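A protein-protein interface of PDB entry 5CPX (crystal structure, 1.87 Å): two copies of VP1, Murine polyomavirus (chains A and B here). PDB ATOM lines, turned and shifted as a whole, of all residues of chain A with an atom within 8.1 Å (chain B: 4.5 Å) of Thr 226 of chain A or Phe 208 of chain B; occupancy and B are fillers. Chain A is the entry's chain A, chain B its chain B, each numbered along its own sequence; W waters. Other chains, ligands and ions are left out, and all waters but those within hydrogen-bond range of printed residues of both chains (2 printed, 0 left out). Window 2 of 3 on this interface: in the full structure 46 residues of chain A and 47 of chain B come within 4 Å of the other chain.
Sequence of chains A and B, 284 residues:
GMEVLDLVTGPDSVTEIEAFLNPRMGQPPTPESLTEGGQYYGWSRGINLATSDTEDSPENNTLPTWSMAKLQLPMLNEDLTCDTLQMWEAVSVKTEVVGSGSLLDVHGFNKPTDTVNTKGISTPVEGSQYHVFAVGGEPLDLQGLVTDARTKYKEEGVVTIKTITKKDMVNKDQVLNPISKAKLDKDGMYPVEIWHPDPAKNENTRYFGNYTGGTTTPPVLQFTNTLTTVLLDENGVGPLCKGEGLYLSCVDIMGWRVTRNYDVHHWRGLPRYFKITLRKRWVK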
ATOM      1  N   LYS A  94      28.175 -35.858  -8.987  1.00  0.00           N
ATOM      2  CA  LYS A  94      27.717 -34.561  -8.514  1.00  0.00           C
ATOM      3  C   LYS A  94      26.881 -33.993  -9.633  1.00  0.00           C
ATOM      4  O   LYS A  94      27.350 -33.861 -10.767  1.00  0.00           O
ATOM      5  CB  LYS A  94      28.904 -33.661  -8.175  1.00  0.00           C
ATOM      6  CG  LYS A  94      29.742 -34.253  -7.058  1.00  0.00           C
ATOM      7  CD  LYS A  94      30.957 -33.400  -6.730  1.00  0.00           C
ATOM      8  CE  LYS A  94      30.637 -32.427  -5.610  1.00  0.00           C
ATOM      9  NZ  LYS A  94      31.866 -31.714  -5.168  1.00  0.00           N
ATOM     10  N   THR A  95      25.612 -33.727  -9.348  1.00  0.00           N
ATOM     11  CA  THR A  95      24.758 -33.185 -10.386  1.00  0.00           C
ATOM     12  C   THR A  95      24.032 -31.938  -9.872  1.00  0.00           C
ATOM     13  O   THR A  95      23.750 -31.828  -8.680  1.00  0.00           O
ATOM     14  CB  THR A  95      23.797 -34.257 -10.962  1.00  0.00           C
ATOM     15  OG1 THR A  95      23.055 -33.694 -12.049  1.00  0.00           O
ATOM     16  CG2 THR A  95      22.826 -34.795  -9.894  1.00  0.00           C
ATOM     17  N   GLU A  96      23.763 -31.004 -10.772  1.00  0.00           N
ATOM     18  CA  GLU A  96      23.177 -29.713 -10.405  1.00  0.00           C
ATOM     19  C   GLU A  96      22.351 -29.184 -11.569  1.00  0.00           C
ATOM     20  O   GLU A  96      22.785 -29.262 -12.721  1.00  0.00           O
ATOM     21  CB  GLU A  96      24.318 -28.727 -10.083  1.00  0.00           C
ATOM     22  CG  GLU A  96      23.885 -27.345  -9.613  1.00  0.00           C
ATOM     23  CD  GLU A  96      25.059 -26.509  -9.099  1.00  0.00           C
ATOM     24  OE1 GLU A  96      26.041 -27.084  -8.577  1.00  0.00           O
ATOM     25  OE2 GLU A  96      24.995 -25.270  -9.227  1.00  0.00           O
ATOM     26  N   GLN A 222      17.063 -26.433  -5.259  1.00  0.00           N
ATOM     27  CA  GLN A 222      18.283 -26.212  -4.486  1.00  0.00           C
ATOM     28  C   GLN A 222      19.462 -26.536  -5.395  1.00  0.00           C
ATOM     29  O   GLN A 222      19.345 -27.373  -6.301  1.00  0.00           O
ATOM     30  CB  GLN A 222      18.321 -27.085  -3.228  1.00  0.00           C
ATOM     31  CG  GLN A 222      17.253 -26.753  -2.192  1.00  0.00           C
ATOM     32  CD  GLN A 222      15.956 -27.519  -2.401  1.00  0.00           C
ATOM     33  OE1 GLN A 222      15.967 -28.712  -2.711  1.00  0.00           O
ATOM     34  NE2 GLN A 222      14.828 -26.838  -2.214  1.00  0.00           N
ATOM     35  N   PHE A 223      20.585 -25.864  -5.166  1.00  0.00           N
ATOM     36  CA  PHE A 223      21.794 -26.102  -5.967  1.00  0.00           C
ATOM     37  C   PHE A 223      23.011 -25.864  -5.087  1.00  0.00           C
ATOM     38  O   PHE A 223      23.039 -24.923  -4.296  1.00  0.00           O
ATOM     39  CB  PHE A 223      21.817 -25.236  -7.256  1.00  0.00           C
ATOM     40  CG  PHE A 223      21.535 -23.764  -7.027  1.00  0.00           C
ATOM     41  CD1 PHE A 223      20.228 -23.306  -6.858  1.00  0.00           C
ATOM     42  CD2 PHE A 223      22.574 -22.832  -7.008  1.00  0.00           C
ATOM     43  CE1 PHE A 223      19.963 -21.957  -6.658  1.00  0.00           C
ATOM     44  CE2 PHE A 223      22.316 -21.474  -6.809  1.00  0.00           C
ATOM     45  CZ  PHE A 223      21.007 -21.040  -6.630  1.00  0.00           C
ATOM     46  N   THR A 224      23.990 -26.759  -5.172  1.00  0.00           N
ATOM     47  CA  THR A 224      25.213 -26.643  -4.394  1.00  0.00           C
ATOM     48  C   THR A 224      26.269 -27.485  -5.092  1.00  0.00           C
ATOM     49  O   THR A 224      25.924 -28.429  -5.803  1.00  0.00           O
ATOM     50  CB  THR A 224      25.030 -27.132  -2.928  1.00  0.00           C
ATOM     51  OG1 THR A 224      26.270 -27.017  -2.219  1.00  0.00           O
ATOM     52  CG2 THR A 224      24.556 -28.580  -2.861  1.00  0.00           C
ATOM     53  N   ASN A 225      27.537 -27.152  -4.886  1.00  0.00           N
ATOM     54  CA  ASN A 225      28.616 -27.974  -5.424  1.00  0.00           C
ATOM     55  C   ASN A 225      29.187 -28.914  -4.353  1.00  0.00           C
ATOM     56  O   ASN A 225      30.288 -29.453  -4.511  1.00  0.00           O
ATOM     57  CB  ASN A 225      29.703 -27.091  -6.078  1.00  0.00           C
ATOM     58  CG  ASN A 225      30.425 -26.178  -5.086  1.00  0.00           C
ATOM     59  OD1 ASN A 225      29.924 -25.865  -3.999  1.00  0.00           O
ATOM     60  ND2 ASN A 225      31.631 -25.751  -5.463  1.00  0.00           N
ATOM     61  N   THR A 226      28.441 -29.101  -3.259  1.00  0.00           N
ATOM     62  CA  THR A 226      28.946 -29.874  -2.115  1.00  0.00           C
ATOM     63  C   THR A 226      28.267 -31.238  -1.922  1.00  0.00           C
ATOM     64  O   THR A 226      28.594 -31.949  -0.973  1.00  0.00           O
ATOM     65  CB  THR A 226      28.777 -29.110  -0.788  1.00  0.00           C
ATOM     66  OG1 THR A 226      27.374 -28.886  -0.547  1.00  0.00           O
ATOM     67  CG2 THR A 226      29.515 -27.774  -0.828  1.00  0.00           C
ATOM     68  N   LEU A 227      27.332 -31.582  -2.803  1.00  0.00           N
ATOM     69  CA  LEU A 227      26.525 -32.800  -2.659  1.00  0.00           C
ATOM     70  C   LEU A 227      26.900 -33.886  -3.668  1.00  0.00           C
ATOM     71  O   LEU A 227      26.827 -33.682  -4.873  1.00  0.00           O
ATOM     72  CB  LEU A 227      25.033 -32.456  -2.785  1.00  0.00           C
ATOM     73  CG  LEU A 227      23.973 -33.560  -2.670  1.00  0.00           C
ATOM     74  CD1 LEU A 227      23.978 -34.207  -1.288  1.00  0.00           C
ATOM     75  CD2 LEU A 227      22.597 -32.998  -3.001  1.00  0.00           C
ATOM     76  N   THR A 228      27.283 -35.046  -3.155  1.00  0.00           N
ATOM     77  CA  THR A 228      27.639 -36.185  -3.973  1.00  0.00           C
ATOM     78  C   THR A 228      26.540 -37.241  -3.861  1.00  0.00           C
ATOM     79  O   THR A 228      26.122 -37.596  -2.751  1.00  0.00           O
ATOM     80  CB  THR A 228      28.968 -36.773  -3.478  1.00  0.00           C
ATOM     81  OG1 THR A 228      29.995 -35.790  -3.639  1.00  0.00           O
ATOM     82  CG2 THR A 228      29.348 -38.047  -4.243  1.00  0.00           C
ATOM     83  N   THR A 229      26.091 -37.744  -5.005  1.00  0.00           N
ATOM     84  CA  THR A 229      25.149 -38.862  -5.045  1.00  0.00           C
ATOM     85  C   THR A 229      25.913 -40.166  -5.273  1.00  0.00           C
ATOM     86  O   THR A 229      26.582 -40.315  -6.299  1.00  0.00           O
ATOM     87  CB  THR A 229      24.132 -38.664  -6.189  1.00  0.00           C
ATOM     88  OG1 THR A 229      23.482 -37.392  -6.049  1.00  0.00           O
ATOM     89  CG2 THR A 229      23.084 -39.768  -6.196  1.00  0.00           C
ATOM     90  N   HIS B 131      18.173 -17.416  -2.134  1.00  0.00           N
ATOM     91  CA  HIS B 131      19.197 -17.321  -1.084  1.00  0.00           C
ATOM     92  C   HIS B 131      20.393 -18.115  -1.527  1.00  0.00           C
ATOM     93  O   HIS B 131      20.286 -19.336  -1.691  1.00  0.00           O
ATOM     94  CB  HIS B 131      18.674 -17.894   0.229  1.00  0.00           C
ATOM     95  CG  HIS B 131      17.552 -17.101   0.806  1.00  0.00           C
ATOM     96  ND1 HIS B 131      17.750 -15.885   1.422  1.00  0.00           N
ATOM     97  CD2 HIS B 131      16.216 -17.312   0.805  1.00  0.00           C
ATOM     98  CE1 HIS B 131      16.586 -15.394   1.805  1.00  0.00           C
ATOM     99  NE2 HIS B 131      15.638 -16.236   1.433  1.00  0.00           N
ATOM    100  N   VAL B 132      21.517 -17.433  -1.745  1.00  0.00           N
ATOM    101  CA  VAL B 132      22.752 -18.128  -2.121  1.00  0.00           C
ATOM    102  C   VAL B 132      23.888 -17.526  -1.312  1.00  0.00           C
ATOM    103  O   VAL B 132      23.932 -16.314  -1.115  1.00  0.00           O
ATOM    104  CB  VAL B 132      23.120 -17.970  -3.622  1.00  0.00           C
ATOM    105  CG1 VAL B 132      24.254 -18.929  -3.994  1.00  0.00           C
ATOM    106  CG2 VAL B 132      21.918 -18.203  -4.514  1.00  0.00           C
ATOM    107  N   PHE B 133      24.782 -18.365  -0.814  1.00  0.00           N
ATOM    108  CA  PHE B 133      26.044 -17.840  -0.286  1.00  0.00           C
ATOM    109  C   PHE B 133      27.199 -18.723  -0.739  1.00  0.00           C
ATOM    110  O   PHE B 133      26.999 -19.899  -1.097  1.00  0.00           O
ATOM    111  CB  PHE B 133      25.988 -17.670   1.242  1.00  0.00           C
ATOM    112  CG  PHE B 133      26.038 -18.963   2.016  1.00  0.00           C
ATOM    113  CD1 PHE B 133      24.876 -19.691   2.265  1.00  0.00           C
ATOM    114  CD2 PHE B 133      27.248 -19.441   2.525  1.00  0.00           C
ATOM    115  CE1 PHE B 133      24.920 -20.876   3.000  1.00  0.00           C
ATOM    116  CE2 PHE B 133      27.298 -20.628   3.255  1.00  0.00           C
ATOM    117  CZ  PHE B 133      26.130 -21.345   3.490  1.00  0.00           C
ATOM    118  N   ARG B 206      33.025 -23.104  -2.070  1.00  0.00           N
ATOM    119  CA  ARG B 206      31.793 -23.842  -1.785  1.00  0.00           C
ATOM    120  C   ARG B 206      30.623 -22.893  -1.884  1.00  0.00           C
ATOM    121  O   ARG B 206      30.678 -21.796  -1.333  1.00  0.00           O
ATOM    122  CB  ARG B 206      31.823 -24.456  -0.386  1.00  0.00           C
ATOM    123  CG  ARG B 206      33.128 -25.152  -0.015  1.00  0.00           C
ATOM    124  CD  ARG B 206      33.441 -26.350  -0.913  1.00  0.00           C
ATOM    125  NE  ARG B 206      34.667 -26.955  -0.415  1.00  0.00           N
ATOM    126  CZ  ARG B 206      35.833 -26.994  -1.045  1.00  0.00           C
ATOM    127  NH1 ARG B 206      35.981 -26.530  -2.284  1.00  0.00           N
ATOM    128  NH2 ARG B 206      36.860 -27.540  -0.425  1.00  0.00           N
ATOM    129  N   TYR B 207      29.562 -23.295  -2.583  1.00  0.00           N
ATOM    130  CA  TYR B 207      28.356 -22.456  -2.650  1.00  0.00           C
ATOM    131  C   TYR B 207      27.104 -23.277  -2.350  1.00  0.00           C
ATOM    132  O   TYR B 207      27.095 -24.506  -2.514  1.00  0.00           O
ATOM    133  CB  TYR B 207      28.240 -21.715  -3.996  1.00  0.00           C
ATOM    134  CG  TYR B 207      28.105 -22.618  -5.216  1.00  0.00           C
ATOM    135  CD1 TYR B 207      26.871 -23.180  -5.582  1.00  0.00           C
ATOM    136  CD2 TYR B 207      29.208 -22.888  -6.013  1.00  0.00           C
ATOM    137  CE1 TYR B 207      26.757 -24.006  -6.704  1.00  0.00           C
ATOM    138  CE2 TYR B 207      29.105 -23.702  -7.131  1.00  0.00           C
ATOM    139  CZ  TYR B 207      27.888 -24.258  -7.464  1.00  0.00           C
ATOM    140  OH  TYR B 207      27.834 -25.056  -8.565  1.00  0.00           O
ATOM    141  N   PHE B 208      26.065 -22.590  -1.871  1.00  0.00           N
ATOM    142  CA  PHE B 208      24.843 -23.237  -1.406  1.00  0.00           C
ATOM    143  C   PHE B 208      23.705 -22.304  -1.788  1.00  0.00           C
ATOM    144  O   PHE B 208      23.668 -21.160  -1.327  1.00  0.00           O
ATOM    145  CB  PHE B 208      24.848 -23.418   0.120  1.00  0.00           C
ATOM    146  CG  PHE B 208      26.103 -24.037   0.676  1.00  0.00           C
ATOM    147  CD1 PHE B 208      27.237 -23.258   0.931  1.00  0.00           C
ATOM    148  CD2 PHE B 208      26.154 -25.398   0.965  1.00  0.00           C
ATOM    149  CE1 PHE B 208      28.397 -23.835   1.449  1.00  0.00           C
ATOM    150  CE2 PHE B 208      27.305 -25.979   1.490  1.00  0.00           C
ATOM    151  CZ  PHE B 208      28.430 -25.197   1.730  1.00  0.00           C
ATOM    152  N   GLY B 209      22.787 -22.774  -2.630  1.00  0.00           N
ATOM    153  CA  GLY B 209      21.707 -21.904  -3.106  1.00  0.00           C
ATOM    154  C   GLY B 209      20.340 -22.550  -3.014  1.00  0.00           C
ATOM    155  O   GLY B 209      20.215 -23.783  -3.063  1.00  0.00           O
ATOM    156  N   THR B 229      28.376 -24.462   9.074  1.00  0.00           N
ATOM    157  CA  THR B 229      28.523 -25.096   7.759  1.00  0.00           C
ATOM    158  C   THR B 229      29.981 -25.527   7.526  1.00  0.00           C
ATOM    159  O   THR B 229      30.877 -24.685   7.505  1.00  0.00           O
ATOM    160  CB  THR B 229      28.089 -24.128   6.641  1.00  0.00           C
ATOM    161  OG1 THR B 229      26.805 -23.572   6.955  1.00  0.00           O
ATOM    162  CG2 THR B 229      28.017 -24.836   5.292  1.00  0.00           C
ATOM    163  N   VAL B 230      30.219 -26.827   7.351  1.00  0.00           N
ATOM    164  CA  VAL B 230      31.577 -27.331   7.071  1.00  0.00           C
ATOM    165  C   VAL B 230      31.970 -26.991   5.626  1.00  0.00           C
ATOM    166  O   VAL B 230      31.145 -27.081   4.719  1.00  0.00           O
ATOM    167  CB  VAL B 230      31.694 -28.849   7.359  1.00  0.00           C
ATOM    168  CG1 VAL B 230      33.038 -29.405   6.888  1.00  0.00           C
ATOM    169  CG2 VAL B 230      31.519 -29.114   8.849  1.00  0.00           C
ATOM    170  N   LEU B 231      33.208 -26.551   5.418  1.00  0.00           N
ATOM    171  CA  LEU B 231      33.659 -26.188   4.064  1.00  0.00           C
ATOM    172  C   LEU B 231      34.662 -27.181   3.468  1.00  0.00           C
ATOM    173  O   LEU B 231      35.070 -27.047   2.308  1.00  0.00           O
ATOM    174  CB  LEU B 231      34.234 -24.764   4.053  1.00  0.00           C
ATOM    175  CG  LEU B 231      33.270 -23.651   4.479  1.00  0.00           C
ATOM    176  CD1 LEU B 231      34.029 -22.353   4.754  1.00  0.00           C
ATOM    177  CD2 LEU B 231      32.198 -23.422   3.419  1.00  0.00           C
HETATM  178  O   HOH W   1      34.618 -27.046  -4.729  1.00  0.00           O
HETATM  179  O   HOH W   2      21.705 -25.739  -1.370  1.00  0.00           O
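The backbone carbonyl oxygen of Tyr 207 of chain B is in hydrogen-bond range of the side-chain hydroxyl of Thr 224 of chain A (2.7 Å). The backbone NH (N) of Tyr 207 of chain B sits at hydrogen-bond distance from the side-chain amide oxygen (OD1) of Asn 225 of chain A, 3.0 Å away. The side-chain carboxylate of Glu 96 of chain A lies within hydrogen-bond range of the side-chain hydroxyl of Tyr 207 of chain B (2.7 Å). The backbone carbonyl oxygen (O) of Phe 223 of chain A lies within hydrogen-bond range of the backbone NH (N) of Gly 209 of chain B, at 2.7 Å.
The backbone carbonyl oxygen of Phe 133 of chain B is in hydrogen-bond range of the backbone NH of Phe 208 of chain B. O of Leu 231 of chain B sits at hydrogen-bond distance from NE of Arg 206 of chain B (2.8 Å). OG1 of Thr 226 of chain A is in hydrogen-bond range of OG1 of Thr 224 of chain A (2.7 Å). The side-chain amino group of Lys 94 of chain A lies within hydrogen-bond range of the backbone carbonyl oxygen of Asn 225 of chain A.
Among the printed residues, pairs that only touch across the chains: Gln 222 of chain A with Gly 209 of chain B (3.4 Å), Phe 223 of chain A with Val 132 of chain B (3.7 Å), Phe 223 of chain A with Phe 208 of chain B (3.7 Å), Thr 224 of chain A with Phe 208 of chain B (3.6 Å), Asn 225 of chain A with Arg 206 of chain B (3.5 Å) and Thr 226 of chain A with Phe 208 of chain B (3.6 Å).
Thr 226 of chain A touches just one residue of chain B: Phe 208. Of chain A, only Phe 223, Thr 224 and Thr 226 come within 4 Å of Phe 208 of chain B. Of the printed residues of chain B, Thr 224 of chain A touches Tyr 207 and Phe 208. Of the printed residues of chain B, Gln 222 of chain A touches Gly 209. Printed residues of chain A within 4 Å of Arg 206 of chain B: Asn 225 (3.5 Å). Printed residues of chain B within 4 Å of Phe 223 of chain A: Val 132 (3.7 Å), Phe 208 (3.7 Å) and Gly 209 (2.7 Å). Of the printed residues of chain B, Glu 96 of chain A touches Tyr 207. Lys 94 of chain A touches none of the printed residues of chain B. The nearest residue of chain B that does not touch Thr 226 of chain A is Arg 206 of chain B (4.1 Å). The nearest residue of chain A that does not touch Phe 208 of chain B is Asn 225 of chain A (5.5 Å).
Hydrophobic or aromatic side chains of chain B that line the printed part of chain A: Val 132, Tyr 207 and Phe 208. Hydrophobic or aromatic side chains of chain A within 4 Å of the printed part of chain B: Phe 223. Along chain A the printed residues that touch a printed residue of chain B span positions 96 to 226. Among the printed residues, 10 pairs touch across the chains. Among the printed residues, no Asp or Glu carboxylate lies within 4 Å of a Lys or Arg side-chain nitrogen of the other chain.
1 position is printed for both chains. Of the 10 pairs that touch across the chains among the printed residues, none has its exchanged pair printed and touching as well.
Water W1 bridges the guanidinium group of Arg 206 of chain B (2.8 Å) and the side-chain amide nitrogen of Asn 225 of chain A (3.3 Å). Water W2 bridges O of Gly 209 of chain B and O of Phe 223 of chain A.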
